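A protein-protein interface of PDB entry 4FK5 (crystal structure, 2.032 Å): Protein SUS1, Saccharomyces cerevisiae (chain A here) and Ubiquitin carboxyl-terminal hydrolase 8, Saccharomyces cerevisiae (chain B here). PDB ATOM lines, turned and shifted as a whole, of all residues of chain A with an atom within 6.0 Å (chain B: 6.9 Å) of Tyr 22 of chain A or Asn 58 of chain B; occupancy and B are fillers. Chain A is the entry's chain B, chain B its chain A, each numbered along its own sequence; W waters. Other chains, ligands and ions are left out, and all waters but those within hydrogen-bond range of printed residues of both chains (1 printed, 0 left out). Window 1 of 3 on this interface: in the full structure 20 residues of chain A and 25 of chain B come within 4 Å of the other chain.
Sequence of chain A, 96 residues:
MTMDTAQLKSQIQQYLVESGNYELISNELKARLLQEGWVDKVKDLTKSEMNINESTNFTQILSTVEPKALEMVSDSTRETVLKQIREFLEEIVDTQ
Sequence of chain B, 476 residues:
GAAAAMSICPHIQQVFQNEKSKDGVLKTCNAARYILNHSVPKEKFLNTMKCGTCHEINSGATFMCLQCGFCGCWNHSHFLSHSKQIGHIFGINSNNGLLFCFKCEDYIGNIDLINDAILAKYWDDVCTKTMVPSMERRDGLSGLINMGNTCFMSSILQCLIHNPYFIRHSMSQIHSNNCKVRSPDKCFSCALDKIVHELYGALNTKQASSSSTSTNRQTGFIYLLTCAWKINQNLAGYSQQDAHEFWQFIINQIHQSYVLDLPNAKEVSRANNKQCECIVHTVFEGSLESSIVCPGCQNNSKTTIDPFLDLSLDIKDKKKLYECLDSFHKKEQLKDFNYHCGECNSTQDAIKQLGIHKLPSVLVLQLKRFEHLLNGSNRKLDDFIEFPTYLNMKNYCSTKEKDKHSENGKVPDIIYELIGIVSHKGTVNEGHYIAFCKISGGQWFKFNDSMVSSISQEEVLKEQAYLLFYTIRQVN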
ATOM      1  N   GLN A  13       1.575   4.233 -15.626  1.00  0.00           N
ATOM      2  CA  GLN A  13       1.660   3.057 -16.519  1.00  0.00           C
ATOM      3  C   GLN A  13       1.875   1.761 -15.766  1.00  0.00           C
ATOM      4  O   GLN A  13       1.281   0.762 -16.100  1.00  0.00           O
ATOM      5  CB  GLN A  13       2.756   3.227 -17.534  1.00  0.00           C
ATOM      6  CG  GLN A  13       2.446   4.340 -18.521  1.00  0.00           C
ATOM      7  CD  GLN A  13       3.526   4.498 -19.555  1.00  0.00           C
ATOM      8  OE1 GLN A  13       3.252   4.434 -20.791  1.00  0.00           O
ATOM      9  NE2 GLN A  13       4.740   4.554 -19.103  1.00  0.00           N
ATOM     10  N   LEU A  16      -1.339   0.815 -14.375  1.00  0.00           N
ATOM     11  CA  LEU A  16      -2.264   0.330 -15.445  1.00  0.00           C
ATOM     12  C   LEU A  16      -1.882  -1.094 -15.830  1.00  0.00           C
ATOM     13  O   LEU A  16      -2.758  -1.979 -15.943  1.00  0.00           O
ATOM     14  CB  LEU A  16      -2.259   1.241 -16.669  1.00  0.00           C
ATOM     15  CG  LEU A  16      -2.935   2.593 -16.541  1.00  0.00           C
ATOM     16  CD1 LEU A  16      -2.638   3.470 -17.775  1.00  0.00           C
ATOM     17  CD2 LEU A  16      -4.421   2.509 -16.284  1.00  0.00           C
ATOM     18  N   VAL A  17      -0.587  -1.382 -15.908  1.00  0.00           N
ATOM     19  CA  VAL A  17      -0.206  -2.726 -16.256  1.00  0.00           C
ATOM     20  C   VAL A  17      -0.585  -3.689 -15.191  1.00  0.00           C
ATOM     21  O   VAL A  17      -1.172  -4.782 -15.486  1.00  0.00           O
ATOM     22  CB  VAL A  17       1.294  -2.865 -16.581  1.00  0.00           C
ATOM     23  CG1 VAL A  17       1.647  -4.338 -16.836  1.00  0.00           C
ATOM     24  CG2 VAL A  17       1.631  -1.999 -17.811  1.00  0.00           C
ATOM     25  N   GLU A  18      -0.188  -3.372 -13.946  1.00  0.00           N
ATOM     26  CA  GLU A  18      -0.340  -4.328 -12.849  1.00  0.00           C
ATOM     27  C   GLU A  18      -1.786  -4.611 -12.543  1.00  0.00           C
ATOM     28  O   GLU A  18      -2.114  -5.741 -12.184  1.00  0.00           O
ATOM     29  CB  GLU A  18       0.420  -3.874 -11.568  1.00  0.00           C
ATOM     30  CG  GLU A  18       1.916  -3.771 -11.782  1.00  0.00           C
ATOM     31  CD  GLU A  18       2.700  -3.454 -10.516  1.00  0.00           C
ATOM     32  OE1 GLU A  18       2.311  -2.524  -9.754  1.00  0.00           O
ATOM     33  OE2 GLU A  18       3.746  -4.112 -10.301  1.00  0.00           O
ATOM     34  N   SER A  19      -2.660  -3.620 -12.738  1.00  0.00           N
ATOM     35  CA  SER A  19      -4.089  -3.790 -12.465  1.00  0.00           C
ATOM     36  C   SER A  19      -4.837  -4.599 -13.577  1.00  0.00           C
ATOM     37  O   SER A  19      -6.048  -4.893 -13.449  1.00  0.00           O
ATOM     38  CB  SER A  19      -4.751  -2.423 -12.351  1.00  0.00           C
ATOM     39  OG  SER A  19      -4.621  -1.670 -13.620  1.00  0.00           O
ATOM     40  N   GLY A  20      -4.179  -4.842 -14.693  1.00  0.00           N
ATOM     41  CA  GLY A  20      -4.812  -5.503 -15.811  1.00  0.00           C
ATOM     42  C   GLY A  20      -5.408  -4.535 -16.840  1.00  0.00           C
ATOM     43  O   GLY A  20      -5.843  -4.947 -17.923  1.00  0.00           O
ATOM     44  N   ASN A  21      -5.427  -3.267 -16.528  1.00  0.00           N
ATOM     45  CA  ASN A  21      -6.098  -2.284 -17.357  1.00  0.00           C
ATOM     46  C   ASN A  21      -5.357  -1.828 -18.613  1.00  0.00           C
ATOM     47  O   ASN A  21      -5.995  -1.501 -19.617  1.00  0.00           O
ATOM     48  CB  ASN A  21      -6.532  -1.100 -16.504  1.00  0.00           C
ATOM     49  CG  ASN A  21      -7.632  -1.492 -15.498  1.00  0.00           C
ATOM     50  OD1 ASN A  21      -8.536  -2.305 -15.831  1.00  0.00           O
ATOM     51  ND2 ASN A  21      -7.468  -1.073 -14.233  1.00  0.00           N
ATOM     52  N   TYR A  22      -4.033  -1.881 -18.595  1.00  0.00           N
ATOM     53  CA  TYR A  22      -3.248  -1.537 -19.761  1.00  0.00           C
ATOM     54  C   TYR A  22      -3.542  -2.520 -20.897  1.00  0.00           C
ATOM     55  O   TYR A  22      -3.692  -2.124 -22.086  1.00  0.00           O
ATOM     56  CB  TYR A  22      -1.752  -1.534 -19.413  1.00  0.00           C
ATOM     57  CG  TYR A  22      -0.881  -0.795 -20.421  1.00  0.00           C
ATOM     58  CD1 TYR A  22      -0.743   0.534 -20.361  1.00  0.00           C
ATOM     59  CD2 TYR A  22      -0.220  -1.478 -21.431  1.00  0.00           C
ATOM     60  CE1 TYR A  22       0.036   1.228 -21.272  1.00  0.00           C
ATOM     61  CE2 TYR A  22       0.595  -0.808 -22.321  1.00  0.00           C
ATOM     62  CZ  TYR A  22       0.715   0.539 -22.243  1.00  0.00           C
ATOM     63  OH  TYR A  22       1.484   1.216 -23.135  1.00  0.00           O
ATOM     64  N   GLU A  23      -3.555  -3.803 -20.568  1.00  0.00           N
ATOM     65  CA  GLU A  23      -3.958  -4.818 -21.545  1.00  0.00           C
ATOM     66  C   GLU A  23      -5.291  -4.485 -22.160  1.00  0.00           C
ATOM     67  O   GLU A  23      -5.468  -4.637 -23.365  1.00  0.00           O
ATOM     68  CB  GLU A  23      -4.111  -6.200 -20.907  1.00  0.00           C
ATOM     69  CG  GLU A  23      -2.846  -6.923 -20.616  1.00  0.00           C
ATOM     70  CD  GLU A  23      -3.073  -8.037 -19.528  1.00  0.00           C
ATOM     71  OE1 GLU A  23      -3.566  -9.118 -19.915  1.00  0.00           O
ATOM     72  OE2 GLU A  23      -2.820  -7.778 -18.320  1.00  0.00           O
ATOM     73  N   LEU A  24      -6.261  -4.116 -21.336  1.00  0.00           N
ATOM     74  CA  LEU A  24      -7.611  -3.793 -21.865  1.00  0.00           C
ATOM     75  C   LEU A  24      -7.561  -2.673 -22.836  1.00  0.00           C
ATOM     76  O   LEU A  24      -8.112  -2.776 -23.945  1.00  0.00           O
ATOM     77  CB  LEU A  24      -8.617  -3.500 -20.775  1.00  0.00           C
ATOM     78  CG  LEU A  24      -8.901  -4.625 -19.808  1.00  0.00           C
ATOM     79  CD1 LEU A  24      -9.854  -4.153 -18.687  1.00  0.00           C
ATOM     80  CD2 LEU A  24      -9.465  -5.890 -20.526  1.00  0.00           C
ATOM     81  N   ILE A  25      -6.805  -1.635 -22.501  1.00  0.00           N
ATOM     82  CA  ILE A  25      -6.742  -0.429 -23.324  1.00  0.00           C
ATOM     83  C   ILE A  25      -6.020  -0.762 -24.631  1.00  0.00           C
ATOM     84  O   ILE A  25      -6.437  -0.359 -25.719  1.00  0.00           O
ATOM     85  CB  ILE A  25      -5.939   0.700 -22.570  1.00  0.00           C
ATOM     86  CG1 ILE A  25      -6.684   1.167 -21.317  1.00  0.00           C
ATOM     87  CG2 ILE A  25      -5.661   1.932 -23.482  1.00  0.00           C
ATOM     88  CD1 ILE A  25      -5.798   1.882 -20.301  1.00  0.00           C
ATOM     89  N   SER A  26      -4.886  -1.431 -24.504  1.00  0.00           N
ATOM     90  CA  SER A  26      -4.096  -1.780 -25.636  1.00  0.00           C
ATOM     91  C   SER A  26      -4.875  -2.655 -26.639  1.00  0.00           C
ATOM     92  O   SER A  26      -4.880  -2.391 -27.826  1.00  0.00           O
ATOM     93  CB  SER A  26      -2.809  -2.512 -25.208  1.00  0.00           C
ATOM     94  OG  SER A  26      -1.965  -2.729 -26.353  1.00  0.00           O
ATOM     95  N   ASN A  27      -5.568  -3.661 -26.151  1.00  0.00           N
ATOM     96  CA  ASN A  27      -6.364  -4.521 -27.042  1.00  0.00           C
ATOM     97  C   ASN A  27      -7.546  -3.797 -27.643  1.00  0.00           C
ATOM     98  O   ASN A  27      -7.954  -4.082 -28.783  1.00  0.00           O
ATOM     99  CB  ASN A  27      -6.869  -5.745 -26.279  1.00  0.00           C
ATOM    100  CG  ASN A  27      -5.745  -6.715 -25.888  1.00  0.00           C
ATOM    101  OD1 ASN A  27      -5.906  -7.520 -24.958  1.00  0.00           O
ATOM    102  ND2 ASN A  27      -4.697  -6.699 -26.608  1.00  0.00           N
ATOM    103  N   PHE B  45       4.909  -6.732 -20.897  1.00  0.00           N
ATOM    104  CA  PHE B  45       4.935  -5.255 -20.737  1.00  0.00           C
ATOM    105  C   PHE B  45       6.029  -4.839 -19.733  1.00  0.00           C
ATOM    106  O   PHE B  45       6.794  -3.947 -20.009  1.00  0.00           O
ATOM    107  CB  PHE B  45       3.566  -4.665 -20.329  1.00  0.00           C
ATOM    108  CG  PHE B  45       2.513  -4.723 -21.421  1.00  0.00           C
ATOM    109  CD1 PHE B  45       2.676  -4.055 -22.600  1.00  0.00           C
ATOM    110  CD2 PHE B  45       1.312  -5.348 -21.198  1.00  0.00           C
ATOM    111  CE1 PHE B  45       1.674  -4.115 -23.599  1.00  0.00           C
ATOM    112  CE2 PHE B  45       0.317  -5.372 -22.172  1.00  0.00           C
ATOM    113  CZ  PHE B  45       0.518  -4.765 -23.373  1.00  0.00           C
ATOM    114  N   MET B  49       9.052  -4.354 -22.454  1.00  0.00           N
ATOM    115  CA  MET B  49       8.556  -3.110 -23.025  1.00  0.00           C
ATOM    116  C   MET B  49       8.661  -1.923 -22.083  1.00  0.00           C
ATOM    117  O   MET B  49       8.017  -0.910 -22.292  1.00  0.00           O
ATOM    118  CB  MET B  49       7.096  -3.300 -23.470  1.00  0.00           C
ATOM    119  CG  MET B  49       7.018  -4.214 -24.666  1.00  0.00           C
ATOM    120  SD  MET B  49       5.352  -4.666 -25.133  1.00  0.00           S
ATOM    121  CE  MET B  49       5.821  -5.795 -26.504  1.00  0.00           C
ATOM    122  N   LYS B  50       9.530  -2.053 -21.085  1.00  0.00           N
ATOM    123  CA  LYS B  50       9.729  -0.997 -20.076  1.00  0.00           C
ATOM    124  C   LYS B  50      11.160  -0.496 -20.218  1.00  0.00           C
ATOM    125  O   LYS B  50      12.100  -1.273 -20.152  1.00  0.00           O
ATOM    126  CB  LYS B  50       9.529  -1.547 -18.677  1.00  0.00           C
ATOM    127  CG  LYS B  50       9.768  -0.489 -17.575  1.00  0.00           C
ATOM    128  CD  LYS B  50       9.879  -1.131 -16.213  1.00  0.00           C
ATOM    129  CE  LYS B  50       9.026  -0.410 -15.174  1.00  0.00           C
ATOM    130  NZ  LYS B  50       9.734  -0.332 -13.849  1.00  0.00           N
ATOM    131  N   CYS B  51      11.324   0.787 -20.480  1.00  0.00           N
ATOM    132  CA  CYS B  51      12.663   1.330 -20.728  1.00  0.00           C
ATOM    133  C   CYS B  51      13.477   1.329 -19.421  1.00  0.00           C
ATOM    134  O   CYS B  51      13.031   1.840 -18.406  1.00  0.00           O
ATOM    135  CB  CYS B  51      12.563   2.748 -21.278  1.00  0.00           C
ATOM    136  SG  CYS B  51      14.214   3.459 -21.640  1.00  0.00           S
ATOM    137  N   GLU B  56       9.326   4.116 -18.743  1.00  0.00           N
ATOM    138  CA  GLU B  56       8.043   4.162 -19.437  1.00  0.00           C
ATOM    139  C   GLU B  56       7.768   2.829 -20.132  1.00  0.00           C
ATOM    140  O   GLU B  56       8.685   2.163 -20.631  1.00  0.00           O
ATOM    141  CB  GLU B  56       8.029   5.258 -20.479  1.00  0.00           C
ATOM    142  CG  GLU B  56       7.696   6.640 -19.944  1.00  0.00           C
ATOM    143  CD  GLU B  56       7.625   7.709 -21.057  1.00  0.00           C
ATOM    144  OE1 GLU B  56       8.162   8.834 -20.842  1.00  0.00           O
ATOM    145  OE2 GLU B  56       6.997   7.463 -22.123  1.00  0.00           O
ATOM    146  N   ILE B  57       6.499   2.517 -20.253  1.00  0.00           N
ATOM    147  CA  ILE B  57       6.048   1.362 -21.002  1.00  0.00           C
ATOM    148  C   ILE B  57       5.771   1.861 -22.414  1.00  0.00           C
ATOM    149  O   ILE B  57       5.066   2.850 -22.585  1.00  0.00           O
ATOM    150  CB  ILE B  57       4.743   0.785 -20.402  1.00  0.00           C
ATOM    151  CG1 ILE B  57       4.882   0.498 -18.868  1.00  0.00           C
ATOM    152  CG2 ILE B  57       4.350  -0.568 -21.104  1.00  0.00           C
ATOM    153  CD1 ILE B  57       6.020  -0.479 -18.559  1.00  0.00           C
ATOM    154  N   ASN B  58       6.243   1.143 -23.418  1.00  0.00           N
ATOM    155  CA  ASN B  58       5.856   1.447 -24.816  1.00  0.00           C
ATOM    156  C   ASN B  58       6.208   2.913 -25.203  1.00  0.00           C
ATOM    157  O   ASN B  58       5.385   3.622 -25.791  1.00  0.00           O
ATOM    158  CB  ASN B  58       4.364   1.256 -25.045  1.00  0.00           C
ATOM    159  CG  ASN B  58       3.906  -0.220 -25.026  1.00  0.00           C
ATOM    160  OD1 ASN B  58       2.744  -0.501 -24.644  1.00  0.00           O
ATOM    161  ND2 ASN B  58       4.773  -1.135 -25.406  1.00  0.00           N
ATOM    162  N   SER B  59       7.385   3.361 -24.829  1.00  0.00           N
ATOM    163  CA  SER B  59       7.946   4.677 -25.301  1.00  0.00           C
ATOM    164  C   SER B  59       8.505   4.490 -26.711  1.00  0.00           C
ATOM    165  O   SER B  59       9.731   4.482 -26.935  1.00  0.00           O
ATOM    166  CB  SER B  59       9.042   5.149 -24.323  1.00  0.00           C
ATOM    167  OG  SER B  59       9.548   6.444 -24.628  1.00  0.00           O
ATOM    168  N   GLY B  60       7.605   4.305 -27.655  1.00  0.00           N
ATOM    169  CA  GLY B  60       7.907   3.633 -28.887  1.00  0.00           C
ATOM    170  C   GLY B  60       8.335   2.207 -28.679  1.00  0.00           C
ATOM    171  O   GLY B  60       8.222   1.693 -27.589  1.00  0.00           O
ATOM    172  N   ALA B  61       8.850   1.568 -29.743  1.00  0.00           N
ATOM    173  CA  ALA B  61       9.541   0.307 -29.613  1.00  0.00           C
ATOM    174  C   ALA B  61      10.516   0.308 -28.424  1.00  0.00           C
ATOM    175  O   ALA B  61      11.289   1.321 -28.186  1.00  0.00           O
ATOM    176  CB  ALA B  61      10.296  -0.046 -30.938  1.00  0.00           C
ATOM    177  N   THR B  62      10.590  -0.844 -27.752  1.00  0.00           N
ATOM    178  CA  THR B  62      11.588  -1.111 -26.742  1.00  0.00           C
ATOM    179  C   THR B  62      12.495  -2.223 -27.276  1.00  0.00           C
ATOM    180  O   THR B  62      12.030  -3.254 -27.875  1.00  0.00           O
ATOM    181  CB  THR B  62      10.922  -1.453 -25.382  1.00  0.00           C
ATOM    182  OG1 THR B  62      10.000  -0.391 -25.005  1.00  0.00           O
ATOM    183  CG2 THR B  62      11.912  -1.621 -24.284  1.00  0.00           C
ATOM    184  N   CYS B  73      14.164   2.372 -24.776  1.00  0.00           N
ATOM    185  CA  CYS B  73      13.118   2.886 -25.707  1.00  0.00           C
ATOM    186  C   CYS B  73      13.674   3.590 -26.948  1.00  0.00           C
ATOM    187  O   CYS B  73      14.836   4.041 -26.994  1.00  0.00           O
ATOM    188  CB  CYS B  73      12.153   3.823 -25.004  1.00  0.00           C
ATOM    189  SG  CYS B  73      12.873   5.474 -24.511  1.00  0.00           S
ATOM    190  N   ASN B  75      11.583   6.293 -28.274  1.00  0.00           N
ATOM    191  CA  ASN B  75      11.079   7.671 -28.425  1.00  0.00           C
ATOM    192  C   ASN B  75      11.962   8.714 -27.727  1.00  0.00           C
ATOM    193  O   ASN B  75      12.039   9.834 -28.192  1.00  0.00           O
ATOM    194  CB  ASN B  75       9.633   7.822 -27.949  1.00  0.00           C
ATOM    195  CG  ASN B  75       8.625   7.272 -28.930  1.00  0.00           C
ATOM    196  OD1 ASN B  75       7.418   7.410 -28.733  1.00  0.00           O
ATOM    197  ND2 ASN B  75       9.085   6.683 -29.949  1.00  0.00           N
ATOM    198  N   SER B  94      10.929  -5.672 -29.053  1.00  0.00           N
ATOM    199  CA  SER B  94      10.183  -6.685 -28.282  1.00  0.00           C
ATOM    200  C   SER B  94       8.711  -6.885 -28.809  1.00  0.00           C
ATOM    201  O   SER B  94       8.025  -7.838 -28.392  1.00  0.00           O
ATOM    202  CB  SER B  94      10.199  -6.361 -26.818  1.00  0.00           C
ATOM    203  OG  SER B  94       9.638  -5.049 -26.568  1.00  0.00           O
ATOM    204  N   ASN B  95       8.283  -6.044 -29.770  1.00  0.00           N
ATOM    205  CA  ASN B  95       7.023  -6.272 -30.469  1.00  0.00           C
ATOM    206  C   ASN B  95       7.109  -7.317 -31.571  1.00  0.00           C
ATOM    207  O   ASN B  95       6.128  -7.882 -31.933  1.00  0.00           O
ATOM    208  CB  ASN B  95       6.488  -4.994 -31.058  1.00  0.00           C
ATOM    209  CG  ASN B  95       5.943  -4.064 -30.008  1.00  0.00           C
ATOM    210  OD1 ASN B  95       4.841  -4.299 -29.461  1.00  0.00           O
ATOM    211  ND2 ASN B  95       6.691  -3.016 -29.695  1.00  0.00           N
HETATM  212  O   HOH W   1       1.010  -1.825 -26.514  1.00  0.00           O
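The backbone NH (N) of Ile 57 of chain B lies close to the side-chain amide nitrogen (NE2) of Gln 13 of chain A.
The side-chain amide oxygen (OD1) of Asn 58 of chain B sits at hydrogen-bond distance from the side-chain hydroxyl (OH) of Tyr 22 of chain A.
The backbone carbonyl oxygen (O) of Phe 45 of chain B is in hydrogen-bond range of the backbone NH (N) of Lys 50 of chain B.
The backbone carbonyl oxygen (O) of Met 49 of chain B is in hydrogen-bond range of the backbone NH (N) of Asn 58 of chain B, 2.9 Å away.
N of Cys 51 of chain B sits at hydrogen-bond distance from O of Glu 56 of chain B, 3.0 Å away.
The backbone carbonyl oxygen (O) of Leu 16 of chain A sits at hydrogen-bond distance from the backbone NH (N) of Tyr 22 of chain A.
OD1 of Asn 27 of chain A lies close to O of Glu 23 of chain A, at 3.3 Å.
CA of Glu 56 of chain B touches NE2 of Gln 13 of chain A (3.3 Å).
Val 17 of chain A touches Phe 45 of chain B.
Tyr 22 of chain A touches Phe 45 of chain B.
Ile 57 of chain B touches Tyr 22 of chain A.
Phe 45 of chain B touches Glu 23 of chain A.
Ser 19 of chain A touches none of the printed residues of chain B.
Tyr 22 of chain A touches three residues of chain B.
Of the printed residues of chain A, Phe 45 of chain B touches Val 17 (3.999 Å), Tyr 22 (3.7 Å) and Glu 23 (3.9 Å).
Met 49 of chain B touches none of the printed residues of chain A.
Printed residues of chain A within 4 Å of Ile 57 of chain B: Gln 13 and Tyr 22.
Of chain A, only Tyr 22 comes within 4 Å of Asn 58 of chain B.
The nearest residue of chain B that does not touch Tyr 22 of chain A is Ser 59 of chain B (6.5 Å).
Of the 13 printed residues of chain A, 4 touch a printed residue of chain B.
Hydrophobic or aromatic side chains of chain A that line the printed part of chain B: Val 17 and Tyr 22.
Of the 15 printed residues of chain B, 4 touch a printed residue of chain A.
Printed residues of chain B that touch a printed residue of chain A: Phe 45, Glu 56, Ile 57 and Asn 58.
Hydrophobic or aromatic side chains of chain B within 4 Å of the printed part of chain A: Phe 45 and Ile 57.
Among the printed residues, 7 pairs touch across the chains.
Among the printed residues, no Asp or Glu carboxylate lies within 4 Å of a Lys or Arg side-chain nitrogen of the other chain.
Water W1 lies within hydrogen-bond range of the side-chain amide oxygen of Asn 58 of chain B (2.9 Å) and the side-chain hydroxyl of Ser 26 of chain A (3.1 Å).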
